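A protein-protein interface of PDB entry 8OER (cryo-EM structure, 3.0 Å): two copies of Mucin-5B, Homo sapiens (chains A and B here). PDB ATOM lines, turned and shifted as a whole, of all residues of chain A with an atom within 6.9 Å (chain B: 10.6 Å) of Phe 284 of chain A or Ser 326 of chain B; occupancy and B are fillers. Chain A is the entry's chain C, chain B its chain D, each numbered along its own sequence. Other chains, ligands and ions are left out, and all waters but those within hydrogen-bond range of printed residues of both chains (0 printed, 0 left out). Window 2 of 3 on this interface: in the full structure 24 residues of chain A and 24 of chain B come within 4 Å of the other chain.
Arg 285 of chain B touches its own counterpart, Arg 285 of chain A. 5 positions are printed for both chains.
The guanidinium group (NH1) of Arg 285 of chain B is in salt-bridge range of the side-chain carboxylate (OD2) of Asp 329 of chain B. SG of Cys 152 of chain B forms a disulfide with SG of Cys 159 of chain B. The guanidinium group of Arg 285 of chain B lies within hydrogen-bond range of the backbone carbonyl oxygen of Ala 321 of chain B. The guanidinium group (NH1) of Arg 285 of chain A is in salt-bridge range of the side-chain carboxylate (OD2) of Asp 329 of chain A (2.8 Å). O of Cys 324 of chain B lies within hydrogen-bond range of NH2 of Arg 285 of chain B, 3.0 Å away. The side-chain sulfur (SG) of Cys 332 of chain B is disulfide-bonded to the side-chain sulfur (SG) of Cys 324 of chain B, at 2.0 Å.
Of the 12 printed residues of chain A, 4 touch a printed residue of chain B. Hydrophobic or aromatic side chains of chain A that line the printed part of chain B: Trp 288. Of the 28 printed residues of chain B, 5 touch a printed residue of chain A. Along chain B the printed residues that touch a printed residue of chain A span positions 285 to 328. Among the printed residues, 9 pairs touch across the chains.
Of chain B, only Ser 326 comes within 4 Å of Phe 284 of chain A. Ser 326 of chain B touches just these residues of chain A: Phe 284 and Trp 288. Arg 285 of chain A touches just these residues of chain B: Arg 285 (3.95 Å), Asp 325 (3.8 Å) and Gly 327 (3.8 Å). Of the printed residues of chain A, Gly 328 of chain B touches Trp 288 (3.5 Å) and Asp 329 (3.98 Å). Of the printed residues of chain B, Asp 329 of chain A touches Gly 327 and Gly 328. Printed residues of chain A within 4 Å of Arg 285 of chain B: Arg 285 (3.95 Å). Cys 324 of chain B touches none of the printed residues of chain A. The nearest residue of chain B that does not touch Phe 284 of chain A is Thr 154 of chain B (5.6 Å).
Among the printed residues, pairs that only touch across the chains: Asp 329 of chain A with Gly 327 of chain B (3.4 Å), Trp 288 of chain A with Gly 328 of chain B (3.5 Å), Trp 288 of chain A with Ser 326 of chain B (3.5 Å), Trp 288 of chain A with Gly 327 of chain B (3.7 Å), Arg 285 of chain A with Asp 325 of chain B (3.8 Å), Arg 285 of chain A with Gly 327 of chain B (3.8 Å), Arg 285 of chain A with Arg 285 of chain B (3.95 Å) and Asp 329 of chain A with Gly 328 of chain B (3.98 Å).
O of Phe 284 of chain A sits at hydrogen-bond distance from OG of Ser 326 of chain B.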
ATOM      1  N   CYS A 279       2.968  -2.156   6.452  1.00  0.00           N
ATOM      2  CA  CYS A 279       1.833  -1.600   5.725  1.00  0.00           C
ATOM      3  C   CYS A 279       1.851  -2.012   4.261  1.00  0.00           C
ATOM      4  O   CYS A 279       0.797  -2.258   3.666  1.00  0.00           O
ATOM      5  CB  CYS A 279       1.824  -0.082   5.859  1.00  0.00           C
ATOM      6  SG  CYS A 279       1.163   0.497   7.433  1.00  0.00           S
ATOM      7  N   ALA A 281       3.045  -4.856   3.237  1.00  0.00           N
ATOM      8  CA  ALA A 281       2.701  -6.272   3.228  1.00  0.00           C
ATOM      9  C   ALA A 281       1.197  -6.483   3.276  1.00  0.00           C
ATOM     10  O   ALA A 281       0.657  -7.331   2.557  1.00  0.00           O
ATOM     11  CB  ALA A 281       3.370  -6.979   4.405  1.00  0.00           C
ATOM     12  N   ASN A 282       0.503  -5.722   4.112  1.00  0.00           N
ATOM     13  CA  ASN A 282      -0.927  -5.901   4.346  1.00  0.00           C
ATOM     14  C   ASN A 282      -1.616  -4.560   4.164  1.00  0.00           C
ATOM     15  O   ASN A 282      -1.946  -3.880   5.142  1.00  0.00           O
ATOM     16  CB  ASN A 282      -1.180  -6.476   5.736  1.00  0.00           C
ATOM     17  CG  ASN A 282      -0.170  -7.526   6.110  1.00  0.00           C
ATOM     18  OD1 ASN A 282      -0.109  -8.588   5.495  1.00  0.00           O
ATOM     19  ND2 ASN A 282       0.640  -7.234   7.113  1.00  0.00           N
ATOM     20  N   PRO A 283      -1.847  -4.148   2.920  1.00  0.00           N
ATOM     21  CA  PRO A 283      -2.433  -2.822   2.691  1.00  0.00           C
ATOM     22  C   PRO A 283      -3.806  -2.658   3.304  1.00  0.00           C
ATOM     23  O   PRO A 283      -4.164  -1.549   3.714  1.00  0.00           O
ATOM     24  CB  PRO A 283      -2.480  -2.730   1.162  1.00  0.00           C
ATOM     25  CG  PRO A 283      -2.583  -4.143   0.717  1.00  0.00           C
ATOM     26  CD  PRO A 283      -1.767  -4.941   1.684  1.00  0.00           C
ATOM     27  N   PHE A 284      -4.583  -3.737   3.396  1.00  0.00           N
ATOM     28  CA  PHE A 284      -5.961  -3.633   3.857  1.00  0.00           C
ATOM     29  C   PHE A 284      -6.067  -3.252   5.326  1.00  0.00           C
ATOM     30  O   PHE A 284      -7.158  -2.901   5.784  1.00  0.00           O
ATOM     31  CB  PHE A 284      -6.689  -4.945   3.591  1.00  0.00           C
ATOM     32  CG  PHE A 284      -6.497  -5.460   2.200  1.00  0.00           C
ATOM     33  CD1 PHE A 284      -6.853  -4.685   1.110  1.00  0.00           C
ATOM     34  CD2 PHE A 284      -5.956  -6.712   1.976  1.00  0.00           C
ATOM     35  CE1 PHE A 284      -6.676  -5.150  -0.178  1.00  0.00           C
ATOM     36  CE2 PHE A 284      -5.776  -7.183   0.688  1.00  0.00           C
ATOM     37  CZ  PHE A 284      -6.138  -6.399  -0.390  1.00  0.00           C
ATOM     38  N   ARG A 285      -4.973  -3.317   6.076  1.00  0.00           N
ATOM     39  CA  ARG A 285      -4.974  -2.810   7.438  1.00  0.00           C
ATOM     40  C   ARG A 285      -4.599  -1.343   7.505  1.00  0.00           C
ATOM     41  O   ARG A 285      -5.031  -0.644   8.429  1.00  0.00           O
ATOM     42  CB  ARG A 285      -3.999  -3.607   8.303  1.00  0.00           C
ATOM     43  CG  ARG A 285      -4.110  -5.102   8.156  1.00  0.00           C
ATOM     44  CD  ARG A 285      -3.280  -5.802   9.199  1.00  0.00           C
ATOM     45  NE  ARG A 285      -4.117  -6.487  10.170  1.00  0.00           N
ATOM     46  CZ  ARG A 285      -4.521  -5.952  11.310  1.00  0.00           C
ATOM     47  NH1 ARG A 285      -4.170  -4.729  11.662  1.00  0.00           N
ATOM     48  NH2 ARG A 285      -5.302  -6.661  12.117  1.00  0.00           N
ATOM     49  N   LYS A 286      -3.827  -0.869   6.523  1.00  0.00           N
ATOM     50  CA  LYS A 286      -3.170   0.428   6.630  1.00  0.00           C
ATOM     51  C   LYS A 286      -4.153   1.520   6.998  1.00  0.00           C
ATOM     52  O   LYS A 286      -3.942   2.259   7.966  1.00  0.00           O
ATOM     53  CB  LYS A 286      -2.470   0.768   5.317  1.00  0.00           C
ATOM     54  CG  LYS A 286      -1.712   2.077   5.346  1.00  0.00           C
ATOM     55  CD  LYS A 286      -0.952   2.293   4.051  1.00  0.00           C
ATOM     56  CE  LYS A 286      -0.168   3.589   4.084  1.00  0.00           C
ATOM     57  NZ  LYS A 286       0.572   3.827   2.820  1.00  0.00           N
ATOM     58  N   SER A 287      -5.261   1.605   6.261  1.00  0.00           N
ATOM     59  CA  SER A 287      -6.249   2.640   6.528  1.00  0.00           C
ATOM     60  C   SER A 287      -6.680   2.607   7.986  1.00  0.00           C
ATOM     61  O   SER A 287      -6.545   3.602   8.711  1.00  0.00           O
ATOM     62  CB  SER A 287      -7.446   2.449   5.604  1.00  0.00           C
ATOM     63  OG  SER A 287      -7.022   2.446   4.256  1.00  0.00           O
ATOM     64  N   TRP A 288      -7.114   1.435   8.453  1.00  0.00           N
ATOM     65  CA  TRP A 288      -7.487   1.302   9.852  1.00  0.00           C
ATOM     66  C   TRP A 288      -6.359   1.788  10.739  1.00  0.00           C
ATOM     67  O   TRP A 288      -6.562   2.644  11.608  1.00  0.00           O
ATOM     68  CB  TRP A 288      -7.831  -0.148  10.177  1.00  0.00           C
ATOM     69  CG  TRP A 288      -8.041  -0.364  11.624  1.00  0.00           C
ATOM     70  CD1 TRP A 288      -9.152  -0.057  12.338  1.00  0.00           C
ATOM     71  CD2 TRP A 288      -7.107  -0.919  12.553  1.00  0.00           C
ATOM     72  NE1 TRP A 288      -8.977  -0.392  13.655  1.00  0.00           N
ATOM     73  CE2 TRP A 288      -7.727  -0.925  13.813  1.00  0.00           C
ATOM     74  CE3 TRP A 288      -5.807  -1.416  12.440  1.00  0.00           C
ATOM     75  CZ2 TRP A 288      -7.093  -1.403  14.953  1.00  0.00           C
ATOM     76  CZ3 TRP A 288      -5.180  -1.892  13.573  1.00  0.00           C
ATOM     77  CH2 TRP A 288      -5.822  -1.882  14.812  1.00  0.00           C
ATOM     78  N   ALA A 289      -5.143   1.306  10.475  1.00  0.00           N
ATOM     79  CA  ALA A 289      -3.999   1.705  11.279  1.00  0.00           C
ATOM     80  C   ALA A 289      -3.913   3.216  11.370  1.00  0.00           C
ATOM     81  O   ALA A 289      -3.863   3.783  12.469  1.00  0.00           O
ATOM     82  CB  ALA A 289      -2.718   1.128  10.687  1.00  0.00           C
ATOM     83  N   CYS A 322      -0.154  -1.981  11.406  1.00  0.00           N
ATOM     84  CA  CYS A 322      -0.189  -2.696  10.135  1.00  0.00           C
ATOM     85  C   CYS A 322       0.301  -4.128  10.284  1.00  0.00           C
ATOM     86  O   CYS A 322      -0.173  -5.026   9.582  1.00  0.00           O
ATOM     87  CB  CYS A 322       0.668  -1.971   9.104  1.00  0.00           C
ATOM     88  SG  CYS A 322      -0.211  -0.901   7.963  1.00  0.00           S
ATOM     89  N   ASP A 329      -4.757  -6.772  18.050  1.00  0.00           N
ATOM     90  CA  ASP A 329      -4.473  -5.492  17.408  1.00  0.00           C
ATOM     91  C   ASP A 329      -4.489  -4.343  18.404  1.00  0.00           C
ATOM     92  O   ASP A 329      -3.649  -3.431  18.333  1.00  0.00           O
ATOM     93  CB  ASP A 329      -5.492  -5.236  16.307  1.00  0.00           C
ATOM     94  CG  ASP A 329      -4.905  -5.391  14.944  1.00  0.00           C
ATOM     95  OD1 ASP A 329      -3.675  -5.543  14.860  1.00  0.00           O
ATOM     96  OD2 ASP A 329      -5.665  -5.369  13.958  1.00  0.00           O
ATOM     97  N   ASP B 108     -20.805 -10.496  13.401  1.00  0.00           N
ATOM     98  CA  ASP B 108     -20.700 -10.443  11.952  1.00  0.00           C
ATOM     99  C   ASP B 108     -22.019 -10.744  11.267  1.00  0.00           C
ATOM    100  O   ASP B 108     -22.045 -10.929  10.047  1.00  0.00           O
ATOM    101  CB  ASP B 108     -19.629 -11.423  11.468  1.00  0.00           C
ATOM    102  CG  ASP B 108     -19.135 -11.109  10.068  1.00  0.00           C
ATOM    103  OD1 ASP B 108     -19.374  -9.981   9.594  1.00  0.00           O
ATOM    104  OD2 ASP B 108     -18.522 -11.992   9.436  1.00  0.00           O
ATOM    105  N   PRO B 151     -18.960   0.101   8.440  1.00  0.00           N
ATOM    106  CA  PRO B 151     -17.524   0.020   8.718  1.00  0.00           C
ATOM    107  C   PRO B 151     -17.049   1.333   9.313  1.00  0.00           C
ATOM    108  O   PRO B 151     -17.327   2.396   8.753  1.00  0.00           O
ATOM    109  CB  PRO B 151     -16.918  -0.254   7.341  1.00  0.00           C
ATOM    110  CG  PRO B 151     -17.872   0.391   6.402  1.00  0.00           C
ATOM    111  CD  PRO B 151     -19.240   0.284   7.009  1.00  0.00           C
ATOM    112  N   CYS B 152     -16.353   1.286  10.446  1.00  0.00           N
ATOM    113  CA  CYS B 152     -16.117   2.495  11.225  1.00  0.00           C
ATOM    114  C   CYS B 152     -14.882   3.279  10.800  1.00  0.00           C
ATOM    115  O   CYS B 152     -14.711   4.416  11.251  1.00  0.00           O
ATOM    116  CB  CYS B 152     -16.015   2.153  12.714  1.00  0.00           C
ATOM    117  SG  CYS B 152     -14.603   1.138  13.171  1.00  0.00           S
ATOM    118  N   GLY B 153     -14.024   2.721   9.954  1.00  0.00           N
ATOM    119  CA  GLY B 153     -12.860   3.465   9.519  1.00  0.00           C
ATOM    120  C   GLY B 153     -12.479   3.233   8.073  1.00  0.00           C
ATOM    121  O   GLY B 153     -11.498   3.796   7.583  1.00  0.00           O
ATOM    122  N   THR B 154     -13.254   2.412   7.378  1.00  0.00           N
ATOM    123  CA  THR B 154     -12.909   1.992   6.028  1.00  0.00           C
ATOM    124  C   THR B 154     -14.199   1.575   5.333  1.00  0.00           C
ATOM    125  O   THR B 154     -15.293   1.951   5.765  1.00  0.00           O
ATOM    126  CB  THR B 154     -11.856   0.872   6.062  1.00  0.00           C
ATOM    127  OG1 THR B 154     -11.449   0.553   4.727  1.00  0.00           O
ATOM    128  CG2 THR B 154     -12.416  -0.372   6.728  1.00  0.00           C
ATOM    129  N   THR B 155     -14.070   0.844   4.227  1.00  0.00           N
ATOM    130  CA  THR B 155     -15.192   0.142   3.607  1.00  0.00           C
ATOM    131  C   THR B 155     -14.759  -1.314   3.489  1.00  0.00           C
ATOM    132  O   THR B 155     -14.250  -1.746   2.453  1.00  0.00           O
ATOM    133  CB  THR B 155     -15.548   0.742   2.270  1.00  0.00           C
ATOM    134  OG1 THR B 155     -14.373   0.801   1.453  1.00  0.00           O
ATOM    135  CG2 THR B 155     -16.092   2.147   2.463  1.00  0.00           C
ATOM    136  N   GLY B 156     -14.960  -2.066   4.565  1.00  0.00           N
ATOM    137  CA  GLY B 156     -14.491  -3.434   4.642  1.00  0.00           C
ATOM    138  C   GLY B 156     -15.321  -4.274   5.585  1.00  0.00           C
ATOM    139  O   GLY B 156     -16.551  -4.279   5.503  1.00  0.00           O
ATOM    140  N   THR B 157     -14.662  -5.003   6.477  1.00  0.00           N
ATOM    141  CA  THR B 157     -15.384  -5.787   7.466  1.00  0.00           C
ATOM    142  C   THR B 157     -16.138  -4.864   8.414  1.00  0.00           C
ATOM    143  O   THR B 157     -15.704  -3.744   8.691  1.00  0.00           O
ATOM    144  CB  THR B 157     -14.421  -6.679   8.241  1.00  0.00           C
ATOM    145  OG1 THR B 157     -13.433  -7.200   7.343  1.00  0.00           O
ATOM    146  CG2 THR B 157     -15.169  -7.840   8.871  1.00  0.00           C
ATOM    147  N   THR B 158     -17.281  -5.339   8.898  1.00  0.00           N
ATOM    148  CA  THR B 158     -18.153  -4.513   9.721  1.00  0.00           C
ATOM    149  C   THR B 158     -17.455  -4.144  11.020  1.00  0.00           C
ATOM    150  O   THR B 158     -16.687  -4.933  11.575  1.00  0.00           O
ATOM    151  CB  THR B 158     -19.444  -5.259  10.027  1.00  0.00           C
ATOM    152  OG1 THR B 158     -19.187  -6.245  11.028  1.00  0.00           O
ATOM    153  CG2 THR B 158     -19.901  -5.985   8.788  1.00  0.00           C
ATOM    154  N   CYS B 159     -17.720  -2.934  11.507  1.00  0.00           N
ATOM    155  CA  CYS B 159     -17.153  -2.470  12.758  1.00  0.00           C
ATOM    156  C   CYS B 159     -18.202  -1.964  13.727  1.00  0.00           C
ATOM    157  O   CYS B 159     -18.003  -2.070  14.939  1.00  0.00           O
ATOM    158  CB  CYS B 159     -16.128  -1.357  12.493  1.00  0.00           C
ATOM    159  SG  CYS B 159     -15.467  -0.528  13.945  1.00  0.00           S
ATOM    160  N   PRO B 278     -14.923 -17.959   7.804  1.00  0.00           N
ATOM    161  CA  PRO B 278     -13.808 -17.057   8.118  1.00  0.00           C
ATOM    162  C   PRO B 278     -12.495 -17.773   8.371  1.00  0.00           C
ATOM    163  O   PRO B 278     -11.460 -17.394   7.819  1.00  0.00           O
ATOM    164  CB  PRO B 278     -14.288 -16.335   9.384  1.00  0.00           C
ATOM    165  CG  PRO B 278     -15.732 -16.678   9.529  1.00  0.00           C
ATOM    166  CD  PRO B 278     -15.907 -18.005   8.891  1.00  0.00           C
ATOM    167  N   ASN B 282      -8.635 -17.309   6.616  1.00  0.00           N
ATOM    168  CA  ASN B 282      -7.476 -16.772   7.322  1.00  0.00           C
ATOM    169  C   ASN B 282      -7.042 -17.773   8.379  1.00  0.00           C
ATOM    170  O   ASN B 282      -7.292 -17.580   9.575  1.00  0.00           O
ATOM    171  CB  ASN B 282      -7.799 -15.418   7.944  1.00  0.00           C
ATOM    172  CG  ASN B 282      -8.690 -14.581   7.064  1.00  0.00           C
ATOM    173  OD1 ASN B 282      -8.311 -14.206   5.959  1.00  0.00           O
ATOM    174  ND2 ASN B 282      -9.884 -14.279   7.551  1.00  0.00           N
ATOM    175  N   ARG B 285      -5.055 -16.617  11.657  1.00  0.00           N
ATOM    176  CA  ARG B 285      -5.741 -16.113  12.835  1.00  0.00           C
ATOM    177  C   ARG B 285      -6.319 -17.233  13.670  1.00  0.00           C
ATOM    178  O   ARG B 285      -6.456 -17.081  14.891  1.00  0.00           O
ATOM    179  CB  ARG B 285      -6.874 -15.171  12.436  1.00  0.00           C
ATOM    180  CG  ARG B 285      -6.515 -14.165  11.379  1.00  0.00           C
ATOM    181  CD  ARG B 285      -7.614 -13.145  11.238  1.00  0.00           C
ATOM    182  NE  ARG B 285      -7.170 -11.827  11.661  1.00  0.00           N
ATOM    183  CZ  ARG B 285      -7.320 -11.351  12.885  1.00  0.00           C
ATOM    184  NH1 ARG B 285      -7.919 -12.054  13.830  1.00  0.00           N
ATOM    185  NH2 ARG B 285      -6.855 -10.142  13.170  1.00  0.00           N
ATOM    186  N   TRP B 288      -5.070 -18.236  17.218  1.00  0.00           N
ATOM    187  CA  TRP B 288      -5.320 -17.155  18.159  1.00  0.00           C
ATOM    188  C   TRP B 288      -6.790 -17.109  18.523  1.00  0.00           C
ATOM    189  O   TRP B 288      -7.148 -17.067  19.705  1.00  0.00           O
ATOM    190  CB  TRP B 288      -4.878 -15.821  17.565  1.00  0.00           C
ATOM    191  CG  TRP B 288      -5.271 -14.651  18.399  1.00  0.00           C
ATOM    192  CD1 TRP B 288      -4.644 -14.204  19.515  1.00  0.00           C
ATOM    193  CD2 TRP B 288      -6.380 -13.776  18.184  1.00  0.00           C
ATOM    194  NE1 TRP B 288      -5.288 -13.103  20.012  1.00  0.00           N
ATOM    195  CE2 TRP B 288      -6.359 -12.817  19.211  1.00  0.00           C
ATOM    196  CE3 TRP B 288      -7.387 -13.707  17.221  1.00  0.00           C
ATOM    197  CZ2 TRP B 288      -7.307 -11.805  19.308  1.00  0.00           C
ATOM    198  CZ3 TRP B 288      -8.325 -12.701  17.317  1.00  0.00           C
ATOM    199  CH2 TRP B 288      -8.281 -11.765  18.354  1.00  0.00           C
ATOM    200  N   ASN B 319     -15.616 -17.761  14.719  1.00  0.00           N
ATOM    201  CA  ASN B 319     -15.775 -17.250  13.363  1.00  0.00           C
ATOM    202  C   ASN B 319     -15.546 -15.746  13.301  1.00  0.00           C
ATOM    203  O   ASN B 319     -14.971 -15.239  12.334  1.00  0.00           O
ATOM    204  CB  ASN B 319     -17.158 -17.606  12.836  1.00  0.00           C
ATOM    205  CG  ASN B 319     -17.309 -19.081  12.585  1.00  0.00           C
ATOM    206  OD1 ASN B 319     -16.329 -19.781  12.350  1.00  0.00           O
ATOM    207  ND2 ASN B 319     -18.538 -19.567  12.640  1.00  0.00           N
ATOM    208  N   ASP B 320     -15.984 -15.015  14.326  1.00  0.00           N
ATOM    209  CA  ASP B 320     -15.782 -13.572  14.340  1.00  0.00           C
ATOM    210  C   ASP B 320     -14.320 -13.216  14.549  1.00  0.00           C
ATOM    211  O   ASP B 320     -13.788 -12.337  13.866  1.00  0.00           O
ATOM    212  CB  ASP B 320     -16.640 -12.939  15.423  1.00  0.00           C
ATOM    213  CG  ASP B 320     -18.056 -12.729  14.979  1.00  0.00           C
ATOM    214  OD1 ASP B 320     -18.380 -13.097  13.832  1.00  0.00           O
ATOM    215  OD2 ASP B 320     -18.849 -12.194  15.776  1.00  0.00           O
ATOM    216  N   ALA B 321     -13.656 -13.877  15.496  1.00  0.00           N
ATOM    217  CA  ALA B 321     -12.234 -13.643  15.685  1.00  0.00           C
ATOM    218  C   ALA B 321     -11.420 -14.049  14.466  1.00  0.00           C
ATOM    219  O   ALA B 321     -10.345 -13.490  14.245  1.00  0.00           O
ATOM    220  CB  ALA B 321     -11.742 -14.391  16.915  1.00  0.00           C
ATOM    221  N   CYS B 322     -11.900 -15.006  13.673  1.00  0.00           N
ATOM    222  CA  CYS B 322     -11.230 -15.346  12.425  1.00  0.00           C
ATOM    223  C   CYS B 322     -11.503 -14.314  11.340  1.00  0.00           C
ATOM    224  O   CYS B 322     -10.643 -14.058  10.493  1.00  0.00           O
ATOM    225  CB  CYS B 322     -11.685 -16.720  11.945  1.00  0.00           C
ATOM    226  SG  CYS B 322     -10.621 -18.101  12.380  1.00  0.00           S
ATOM    227  N   ALA B 323     -12.699 -13.729  11.337  1.00  0.00           N
ATOM    228  CA  ALA B 323     -13.110 -12.872  10.232  1.00  0.00           C
ATOM    229  C   ALA B 323     -12.471 -11.491  10.294  1.00  0.00           C
ATOM    230  O   ALA B 323     -12.140 -10.915   9.255  1.00  0.00           O
ATOM    231  CB  ALA B 323     -14.632 -12.742  10.211  1.00  0.00           C
ATOM    232  N   CYS B 324     -12.289 -10.940  11.493  1.00  0.00           N
ATOM    233  CA  CYS B 324     -11.866  -9.548  11.639  1.00  0.00           C
ATOM    234  C   CYS B 324     -10.386  -9.418  11.278  1.00  0.00           C
ATOM    235  O   CYS B 324      -9.515  -9.194  12.118  1.00  0.00           O
ATOM    236  CB  CYS B 324     -12.140  -9.059  13.053  1.00  0.00           C
ATOM    237  SG  CYS B 324     -13.871  -9.174  13.532  1.00  0.00           S
ATOM    238  N   ASP B 325     -10.112  -9.553   9.984  1.00  0.00           N
ATOM    239  CA  ASP B 325      -8.750  -9.477   9.480  1.00  0.00           C
ATOM    240  C   ASP B 325      -8.347  -8.076   9.050  1.00  0.00           C
ATOM    241  O   ASP B 325      -7.241  -7.901   8.531  1.00  0.00           O
ATOM    242  CB  ASP B 325      -8.564 -10.429   8.298  1.00  0.00           C
ATOM    243  CG  ASP B 325      -9.507 -10.130   7.159  1.00  0.00           C
ATOM    244  OD1 ASP B 325     -10.444  -9.332   7.357  1.00  0.00           O
ATOM    245  OD2 ASP B 325      -9.312 -10.690   6.061  1.00  0.00           O
ATOM    246  N   SER B 326      -9.210  -7.084   9.236  1.00  0.00           N
ATOM    247  CA  SER B 326      -8.898  -5.729   8.813  1.00  0.00           C
ATOM    248  C   SER B 326      -8.742  -4.754   9.968  1.00  0.00           C
ATOM    249  O   SER B 326      -8.656  -3.548   9.727  1.00  0.00           O
ATOM    250  CB  SER B 326      -9.975  -5.205   7.868  1.00  0.00           C
ATOM    251  OG  SER B 326      -9.678  -3.883   7.465  1.00  0.00           O
ATOM    252  N   GLY B 327      -8.723  -5.227  11.198  1.00  0.00           N
ATOM    253  CA  GLY B 327      -8.486  -4.370  12.343  1.00  0.00           C
ATOM    254  C   GLY B 327      -9.648  -4.421  13.311  1.00  0.00           C
ATOM    255  O   GLY B 327     -10.771  -4.781  12.963  1.00  0.00           O
ATOM    256  N   GLY B 328      -9.373  -4.036  14.553  1.00  0.00           N
ATOM    257  CA  GLY B 328     -10.376  -4.100  15.593  1.00  0.00           C
ATOM    258  C   GLY B 328     -10.713  -5.530  15.949  1.00  0.00           C
ATOM    259  O   GLY B 328     -11.823  -5.994  15.684  1.00  0.00           O
ATOM    260  N   ASP B 329      -9.753  -6.247  16.534  1.00  0.00           N
ATOM    261  CA  ASP B 329      -9.961  -7.653  16.863  1.00  0.00           C
ATOM    262  C   ASP B 329     -10.584  -7.828  18.239  1.00  0.00           C
ATOM    263  O   ASP B 329     -11.513  -8.634  18.415  1.00  0.00           O
ATOM    264  CB  ASP B 329      -8.636  -8.401  16.799  1.00  0.00           C
ATOM    265  CG  ASP B 329      -8.553  -9.315  15.616  1.00  0.00           C
ATOM    266  OD1 ASP B 329      -9.570  -9.450  14.912  1.00  0.00           O
ATOM    267  OD2 ASP B 329      -7.478  -9.900  15.389  1.00  0.00           O
ATOM    268  N   CYS B 330     -10.074  -7.094  19.225  1.00  0.00           N
ATOM    269  CA  CYS B 330     -10.579  -7.252  20.577  1.00  0.00           C
ATOM    270  C   CYS B 330     -12.054  -6.921  20.639  1.00  0.00           C
ATOM    271  O   CYS B 330     -12.793  -7.534  21.403  1.00  0.00           O
ATOM    272  CB  CYS B 330      -9.799  -6.376  21.545  1.00  0.00           C
ATOM    273  SG  CYS B 330      -8.093  -6.151  21.073  1.00  0.00           S
ATOM    274  N   GLU B 331     -12.509  -5.961  19.837  1.00  0.00           N
ATOM    275  CA  GLU B 331     -13.931  -5.639  19.828  1.00  0.00           C
ATOM    276  C   GLU B 331     -14.759  -6.811  19.317  1.00  0.00           C
ATOM    277  O   GLU B 331     -15.819  -7.119  19.874  1.00  0.00           O
ATOM    278  CB  GLU B 331     -14.186  -4.390  18.987  1.00  0.00           C
ATOM    279  CG  GLU B 331     -13.338  -3.169  19.355  1.00  0.00           C
ATOM    280  CD  GLU B 331     -11.904  -3.235  18.846  1.00  0.00           C
ATOM    281  OE1 GLU B 331     -11.464  -2.265  18.195  1.00  0.00           O
ATOM    282  OE2 GLU B 331     -11.212  -4.243  19.107  1.00  0.00           O
ATOM    283  N   CYS B 332     -14.287  -7.484  18.266  1.00  0.00           N
ATOM    284  CA  CYS B 332     -15.000  -8.645  17.743  1.00  0.00           C
ATOM    285  C   CYS B 332     -15.112  -9.735  18.797  1.00  0.00           C
ATOM    286  O   CYS B 332     -16.210 -10.231  19.089  1.00  0.00           O
ATOM    287  CB  CYS B 332     -14.286  -9.189  16.510  1.00  0.00           C
ATOM    288  SG  CYS B 332     -14.027  -8.011  15.187  1.00  0.00           S
